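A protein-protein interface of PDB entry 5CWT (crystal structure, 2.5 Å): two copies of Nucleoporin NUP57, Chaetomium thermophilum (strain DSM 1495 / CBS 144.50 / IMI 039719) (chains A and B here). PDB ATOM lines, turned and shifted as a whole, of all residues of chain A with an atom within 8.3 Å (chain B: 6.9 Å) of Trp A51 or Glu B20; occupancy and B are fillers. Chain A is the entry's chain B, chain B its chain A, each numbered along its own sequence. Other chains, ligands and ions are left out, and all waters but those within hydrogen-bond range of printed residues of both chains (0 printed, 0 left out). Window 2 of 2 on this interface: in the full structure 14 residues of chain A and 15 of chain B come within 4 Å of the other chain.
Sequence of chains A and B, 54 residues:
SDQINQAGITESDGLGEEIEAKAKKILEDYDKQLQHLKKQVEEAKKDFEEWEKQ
Hydrophobic or aromatic side chains of chain A within 4 Å of the printed part of chain B: Phe A48 and Trp A51.
Of the 12 printed residues of chain B, 4 touch a printed residue of chain A.
Along chain B the printed residues that touch a printed residue of chain A span positions 20 to 27.
Among the printed residues, 8 pairs touch across the chains.
Among the printed residues, no Asp or Glu carboxylate lies within 4 Å of a Lys or Arg side-chain nitrogen of the other chain.
The side-chain amino group (NZ) of Lys B24 lies within salt-bridge range of the side-chain carboxylate (OE2) of Glu B20 (3.6 Å).
No position is printed for both chains.
Trp A51 touches just these residues of chain B: Glu B20, Ala B23, Lys B24 and Leu B27.
Glu B20 touches just one residue of chain A: Trp A51.
Printed residues of chain B within 4 Å of Asp A47: Leu B27 (3.8 Å).
Printed residues of chain B within 4 Å of Ala A44: Leu B27.
Of the printed residues of chain A, Lys B24 touches Phe A48 and Trp A51.
Of the printed residues of chain A, Leu B27 touches Ala A44, Asp A47, Phe A48 and Trp A51.
Printed residues of chain A within 4 Å of Ala B23: Trp A51 (3.2 Å).
Ile B19 touches none of the printed residues of chain A.
The nearest residue of chain B that does not touch Trp A51 is Ile B19 (4.5 Å).
The nearest residue of chain A that does not touch Glu B20 is Glu A52 (4.3 Å).
The nearest printed residue of chain B that does not touch Ala A44 is Ala B23 (7.6 Å).
The side-chain carboxylate (OE2) of Glu B20 sits close to the backbone carbonyl oxygen (O) of Trp A51 (3.2 Å).
Ala A44 touches Leu B27.
C of Asp A47 touches CD1 of Leu B27, 3.8 Å away.
Lys B24 touches Phe A48.
Phe A48 touches Leu B27 (N to CD1, 3.6 Å).
Ala B23 touches Trp A51.
CB of Trp A51 touches CG of Lys B24 (3.9 Å).
Trp A51 touches Leu B27 (CD1 to CD1, 3.6 Å).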
ATOM      1  N   ALA A  44     -22.345  10.952 -13.117  1.00  0.00           N
ATOM      2  CA  ALA A  44     -22.673  12.351 -13.355  1.00  0.00           C
ATOM      3  C   ALA A  44     -22.959  13.054 -12.036  1.00  0.00           C
ATOM      4  O   ALA A  44     -22.708  14.251 -11.893  1.00  0.00           O
ATOM      5  CB  ALA A  44     -23.869  12.465 -14.286  1.00  0.00           C
ATOM      6  N   LYS A  45     -23.480  12.303 -11.073  1.00  0.00           N
ATOM      7  CA  LYS A  45     -23.826  12.863  -9.775  1.00  0.00           C
ATOM      8  C   LYS A  45     -22.570  13.229  -8.990  1.00  0.00           C
ATOM      9  O   LYS A  45     -22.485  14.313  -8.416  1.00  0.00           O
ATOM     10  CB  LYS A  45     -24.671  11.867  -8.979  1.00  0.00           C
ATOM     11  CG  LYS A  45     -25.521  12.506  -7.895  1.00  0.00           C
ATOM     12  CD  LYS A  45     -27.008  12.298  -8.157  1.00  0.00           C
ATOM     13  CE  LYS A  45     -27.450  10.885  -7.809  1.00  0.00           C
ATOM     14  NZ  LYS A  45     -28.845  10.609  -8.259  1.00  0.00           N
ATOM     15  N   LYS A  46     -21.592  12.326  -8.973  1.00  0.00           N
ATOM     16  CA  LYS A  46     -20.371  12.554  -8.208  1.00  0.00           C
ATOM     17  C   LYS A  46     -19.518  13.652  -8.845  1.00  0.00           C
ATOM     18  O   LYS A  46     -18.806  14.375  -8.148  1.00  0.00           O
ATOM     19  CB  LYS A  46     -19.571  11.253  -8.046  1.00  0.00           C
ATOM     20  CG  LYS A  46     -18.700  10.868  -9.234  1.00  0.00           C
ATOM     21  CD  LYS A  46     -18.080   9.488  -9.039  1.00  0.00           C
ATOM     22  CE  LYS A  46     -17.315   9.032 -10.273  1.00  0.00           C
ATOM     23  NZ  LYS A  46     -16.704   7.687 -10.098  1.00  0.00           N
ATOM     24  N   ASP A  47     -19.595  13.780 -10.166  1.00  0.00           N
ATOM     25  CA  ASP A  47     -18.909  14.863 -10.865  1.00  0.00           C
ATOM     26  C   ASP A  47     -19.542  16.202 -10.513  1.00  0.00           C
ATOM     27  O   ASP A  47     -18.849  17.203 -10.344  1.00  0.00           O
ATOM     28  CB  ASP A  47     -18.971  14.658 -12.379  1.00  0.00           C
ATOM     29  CG  ASP A  47     -18.021  13.586 -12.866  1.00  0.00           C
ATOM     30  OD1 ASP A  47     -16.910  13.468 -12.308  1.00  0.00           O
ATOM     31  OD2 ASP A  47     -18.385  12.862 -13.815  1.00  0.00           O
ATOM     32  N   PHE A  48     -20.867  16.209 -10.414  1.00  0.00           N
ATOM     33  CA  PHE A  48     -21.613  17.419 -10.088  1.00  0.00           C
ATOM     34  C   PHE A  48     -21.291  17.879  -8.671  1.00  0.00           C
ATOM     35  O   PHE A  48     -21.128  19.072  -8.416  1.00  0.00           O
ATOM     36  CB  PHE A  48     -23.111  17.154 -10.225  1.00  0.00           C
ATOM     37  CG  PHE A  48     -23.966  18.375 -10.063  1.00  0.00           C
ATOM     38  CD1 PHE A  48     -24.155  19.248 -11.120  1.00  0.00           C
ATOM     39  CD2 PHE A  48     -24.595  18.642  -8.859  1.00  0.00           C
ATOM     40  CE1 PHE A  48     -24.951  20.368 -10.978  1.00  0.00           C
ATOM     41  CE2 PHE A  48     -25.392  19.762  -8.710  1.00  0.00           C
ATOM     42  CZ  PHE A  48     -25.569  20.626  -9.771  1.00  0.00           C
ATOM     43  N   GLU A  49     -21.203  16.924  -7.751  1.00  0.00           N
ATOM     44  CA  GLU A  49     -20.869  17.225  -6.366  1.00  0.00           C
ATOM     45  C   GLU A  49     -19.440  17.746  -6.258  1.00  0.00           C
ATOM     46  O   GLU A  49     -19.135  18.563  -5.390  1.00  0.00           O
ATOM     47  CB  GLU A  49     -21.045  15.983  -5.491  1.00  0.00           C
ATOM     48  CG  GLU A  49     -22.489  15.522  -5.350  1.00  0.00           C
ATOM     49  CD  GLU A  49     -22.602  14.146  -4.722  1.00  0.00           C
ATOM     50  OE1 GLU A  49     -21.613  13.688  -4.112  1.00  0.00           O
ATOM     51  OE2 GLU A  49     -23.677  13.520  -4.841  1.00  0.00           O
ATOM     52  N   GLU A  50     -18.567  17.280  -7.144  1.00  0.00           N
ATOM     53  CA  GLU A  50     -17.173  17.705  -7.125  1.00  0.00           C
ATOM     54  C   GLU A  50     -17.008  19.123  -7.668  1.00  0.00           C
ATOM     55  O   GLU A  50     -16.081  19.834  -7.285  1.00  0.00           O
ATOM     56  CB  GLU A  50     -16.307  16.733  -7.922  1.00  0.00           C
ATOM     57  CG  GLU A  50     -14.819  17.010  -7.805  1.00  0.00           C
ATOM     58  CD  GLU A  50     -13.973  15.914  -8.423  1.00  0.00           C
ATOM     59  OE1 GLU A  50     -14.499  14.799  -8.627  1.00  0.00           O
ATOM     60  OE2 GLU A  50     -12.784  16.170  -8.711  1.00  0.00           O
ATOM     61  N   TRP A  51     -17.905  19.528  -8.564  1.00  0.00           N
ATOM     62  CA  TRP A  51     -17.898  20.889  -9.093  1.00  0.00           C
ATOM     63  C   TRP A  51     -18.419  21.874  -8.055  1.00  0.00           C
ATOM     64  O   TRP A  51     -18.094  23.061  -8.093  1.00  0.00           O
ATOM     65  CB  TRP A  51     -18.743  20.978 -10.362  1.00  0.00           C
ATOM     66  CG  TRP A  51     -18.002  20.577 -11.593  1.00  0.00           C
ATOM     67  CD1 TRP A  51     -18.182  19.445 -12.329  1.00  0.00           C
ATOM     68  CD2 TRP A  51     -16.951  21.310 -12.233  1.00  0.00           C
ATOM     69  NE1 TRP A  51     -17.310  19.428 -13.390  1.00  0.00           N
ATOM     70  CE2 TRP A  51     -16.546  20.563 -13.355  1.00  0.00           C
ATOM     71  CE3 TRP A  51     -16.317  22.524 -11.967  1.00  0.00           C
ATOM     72  CZ2 TRP A  51     -15.530  20.990 -14.207  1.00  0.00           C
ATOM     73  CZ3 TRP A  51     -15.314  22.949 -12.814  1.00  0.00           C
ATOM     74  CH2 TRP A  51     -14.929  22.183 -13.921  1.00  0.00           C
ATOM     75  N   GLU A  52     -19.224  21.369  -7.125  1.00  0.00           N
ATOM     76  CA  GLU A  52     -19.703  22.165  -6.002  1.00  0.00           C
ATOM     77  C   GLU A  52     -18.652  22.177  -4.897  1.00  0.00           C
ATOM     78  O   GLU A  52     -18.938  22.576  -3.769  1.00  0.00           O
ATOM     79  CB  GLU A  52     -21.022  21.596  -5.471  1.00  0.00           C
ATOM     80  CG  GLU A  52     -22.168  21.637  -6.476  1.00  0.00           C
ATOM     81  CD  GLU A  52     -23.394  20.872  -6.008  1.00  0.00           C
ATOM     82  OE1 GLU A  52     -23.399  19.627  -6.115  1.00  0.00           O
ATOM     83  OE2 GLU A  52     -24.351  21.513  -5.531  1.00  0.00           O
ATOM     84  N   LYS A  53     -17.443  21.727  -5.236  1.00  0.00           N
ATOM     85  CA  LYS A  53     -16.320  21.668  -4.306  1.00  0.00           C
ATOM     86  C   LYS A  53     -16.547  20.607  -3.231  1.00  0.00           C
ATOM     87  O   LYS A  53     -15.597  20.109  -2.627  1.00  0.00           O
ATOM     88  CB  LYS A  53     -16.064  23.035  -3.669  1.00  0.00           C
ATOM     89  CG  LYS A  53     -14.741  23.128  -2.934  1.00  0.00           C
ATOM     90  CD  LYS A  53     -14.470  24.534  -2.427  1.00  0.00           C
ATOM     91  CE  LYS A  53     -15.639  25.074  -1.624  1.00  0.00           C
ATOM     92  NZ  LYS A  53     -15.248  26.195  -0.728  1.00  0.00           N
ATOM     93  N   LEU B  15     -13.733  34.167 -13.567  1.00  0.00           N
ATOM     94  CA  LEU B  15     -14.264  33.188 -14.510  1.00  0.00           C
ATOM     95  C   LEU B  15     -14.466  31.830 -13.856  1.00  0.00           C
ATOM     96  O   LEU B  15     -15.227  31.005 -14.358  1.00  0.00           O
ATOM     97  CB  LEU B  15     -13.317  33.026 -15.696  1.00  0.00           C
ATOM     98  CG  LEU B  15     -13.112  34.251 -16.584  1.00  0.00           C
ATOM     99  CD1 LEU B  15     -12.045  33.953 -17.609  1.00  0.00           C
ATOM    100  CD2 LEU B  15     -14.405  34.657 -17.272  1.00  0.00           C
ATOM    101  N   GLY B  16     -13.770  31.604 -12.746  1.00  0.00           N
ATOM    102  CA  GLY B  16     -13.845  30.344 -12.029  1.00  0.00           C
ATOM    103  C   GLY B  16     -15.268  29.912 -11.742  1.00  0.00           C
ATOM    104  O   GLY B  16     -15.633  28.760 -11.970  1.00  0.00           O
ATOM    105  N   GLU B  17     -16.080  30.842 -11.251  1.00  0.00           N
ATOM    106  CA  GLU B  17     -17.470  30.547 -10.933  1.00  0.00           C
ATOM    107  C   GLU B  17     -18.307  30.375 -12.196  1.00  0.00           C
ATOM    108  O   GLU B  17     -19.305  29.655 -12.196  1.00  0.00           O
ATOM    109  CB  GLU B  17     -18.062  31.658 -10.065  1.00  0.00           C
ATOM    110  CG  GLU B  17     -17.459  31.732  -8.674  1.00  0.00           C
ATOM    111  CD  GLU B  17     -18.058  32.844  -7.835  1.00  0.00           C
ATOM    112  OE1 GLU B  17     -18.697  33.750  -8.411  1.00  0.00           O
ATOM    113  OE2 GLU B  17     -17.894  32.809  -6.597  1.00  0.00           O
ATOM    114  N   GLU B  18     -17.899  31.043 -13.272  1.00  0.00           N
ATOM    115  CA  GLU B  18     -18.617  30.963 -14.538  1.00  0.00           C
ATOM    116  C   GLU B  18     -18.344  29.617 -15.210  1.00  0.00           C
ATOM    117  O   GLU B  18     -19.251  28.991 -15.759  1.00  0.00           O
ATOM    118  CB  GLU B  18     -18.209  32.123 -15.452  1.00  0.00           C
ATOM    119  CG  GLU B  18     -19.116  32.320 -16.665  1.00  0.00           C
ATOM    120  CD  GLU B  18     -18.499  31.835 -17.968  1.00  0.00           C
ATOM    121  OE1 GLU B  18     -17.665  30.905 -17.940  1.00  0.00           O
ATOM    122  OE2 GLU B  18     -18.855  32.392 -19.029  1.00  0.00           O
ATOM    123  N   ILE B  19     -17.089  29.182 -15.158  1.00  0.00           N
ATOM    124  CA  ILE B  19     -16.702  27.863 -15.642  1.00  0.00           C
ATOM    125  C   ILE B  19     -17.451  26.797 -14.850  1.00  0.00           C
ATOM    126  O   ILE B  19     -18.034  25.876 -15.424  1.00  0.00           O
ATOM    127  CB  ILE B  19     -15.184  27.640 -15.482  1.00  0.00           C
ATOM    128  CG1 ILE B  19     -14.408  28.620 -16.361  1.00  0.00           C
ATOM    129  CG2 ILE B  19     -14.793  26.210 -15.848  1.00  0.00           C
ATOM    130  CD1 ILE B  19     -12.965  28.805 -15.941  1.00  0.00           C
ATOM    131  N   GLU B  20     -17.424  26.935 -13.528  1.00  0.00           N
ATOM    132  CA  GLU B  20     -18.106  26.011 -12.633  1.00  0.00           C
ATOM    133  C   GLU B  20     -19.590  25.923 -12.967  1.00  0.00           C
ATOM    134  O   GLU B  20     -20.168  24.836 -12.978  1.00  0.00           O
ATOM    135  CB  GLU B  20     -17.925  26.464 -11.182  1.00  0.00           C
ATOM    136  CG  GLU B  20     -18.628  25.595 -10.152  1.00  0.00           C
ATOM    137  CD  GLU B  20     -18.450  26.113  -8.740  1.00  0.00           C
ATOM    138  OE1 GLU B  20     -17.372  26.672  -8.443  1.00  0.00           O
ATOM    139  OE2 GLU B  20     -19.390  25.971  -7.930  1.00  0.00           O
ATOM    140  N   ALA B  21     -20.199  27.071 -13.243  1.00  0.00           N
ATOM    141  CA  ALA B  21     -21.621  27.129 -13.567  1.00  0.00           C
ATOM    142  C   ALA B  21     -21.935  26.344 -14.838  1.00  0.00           C
ATOM    143  O   ALA B  21     -22.919  25.606 -14.892  1.00  0.00           O
ATOM    144  CB  ALA B  21     -22.065  28.572 -13.719  1.00  0.00           C
ATOM    145  N   LYS B  22     -21.096  26.508 -15.858  1.00  0.00           N
ATOM    146  CA  LYS B  22     -21.280  25.804 -17.121  1.00  0.00           C
ATOM    147  C   LYS B  22     -21.091  24.308 -16.942  1.00  0.00           C
ATOM    148  O   LYS B  22     -21.865  23.507 -17.462  1.00  0.00           O
ATOM    149  CB  LYS B  22     -20.283  26.300 -18.162  1.00  0.00           C
ATOM    150  CG  LYS B  22     -20.559  27.689 -18.677  1.00  0.00           C
ATOM    151  CD  LYS B  22     -19.487  28.108 -19.662  1.00  0.00           C
ATOM    152  CE  LYS B  22     -19.763  29.480 -20.230  1.00  0.00           C
ATOM    153  NZ  LYS B  22     -21.020  29.528 -21.027  1.00  0.00           N
ATOM    154  N   ALA B  23     -20.043  23.935 -16.217  1.00  0.00           N
ATOM    155  CA  ALA B  23     -19.733  22.530 -16.005  1.00  0.00           C
ATOM    156  C   ALA B  23     -20.887  21.831 -15.300  1.00  0.00           C
ATOM    157  O   ALA B  23     -21.176  20.666 -15.569  1.00  0.00           O
ATOM    158  CB  ALA B  23     -18.468  22.385 -15.201  1.00  0.00           C
ATOM    159  N   LYS B  24     -21.542  22.545 -14.394  1.00  0.00           N
ATOM    160  CA  LYS B  24     -22.722  22.018 -13.729  1.00  0.00           C
ATOM    161  C   LYS B  24     -23.897  21.945 -14.702  1.00  0.00           C
ATOM    162  O   LYS B  24     -24.717  21.030 -14.627  1.00  0.00           O
ATOM    163  CB  LYS B  24     -23.078  22.875 -12.513  1.00  0.00           C
ATOM    164  CG  LYS B  24     -22.132  22.677 -11.338  1.00  0.00           C
ATOM    165  CD  LYS B  24     -22.613  23.397 -10.085  1.00  0.00           C
ATOM    166  CE  LYS B  24     -22.608  24.904 -10.257  1.00  0.00           C
ATOM    167  NZ  LYS B  24     -22.848  25.607  -8.966  1.00  0.00           N
ATOM    168  N   LYS B  25     -23.972  22.903 -15.621  1.00  0.00           N
ATOM    169  CA  LYS B  25     -25.038  22.920 -16.619  1.00  0.00           C
ATOM    170  C   LYS B  25     -24.903  21.738 -17.579  1.00  0.00           C
ATOM    171  O   LYS B  25     -25.891  21.090 -17.922  1.00  0.00           O
ATOM    172  CB  LYS B  25     -25.022  24.240 -17.396  1.00  0.00           C
ATOM    173  CG  LYS B  25     -26.052  24.333 -18.518  1.00  0.00           C
ATOM    174  CD  LYS B  25     -27.475  24.165 -18.002  1.00  0.00           C
ATOM    175  CE  LYS B  25     -28.492  24.310 -19.124  1.00  0.00           C
ATOM    176  NZ  LYS B  25     -29.884  24.069 -18.652  1.00  0.00           N
ATOM    177  N   LEU B  27     -23.518  18.867 -16.969  1.00  0.00           N
ATOM    178  CA  LEU B  27     -23.854  17.645 -16.249  1.00  0.00           C
ATOM    179  C   LEU B  27     -25.360  17.510 -16.043  1.00  0.00           C
ATOM    180  O   LEU B  27     -25.893  16.401 -16.024  1.00  0.00           O
ATOM    181  CB  LEU B  27     -23.129  17.607 -14.905  1.00  0.00           C
ATOM    182  CG  LEU B  27     -21.657  17.205 -14.994  1.00  0.00           C
ATOM    183  CD1 LEU B  27     -20.910  17.612 -13.735  1.00  0.00           C
ATOM    184  CD2 LEU B  27     -21.535  15.706 -15.229  1.00  0.00           C
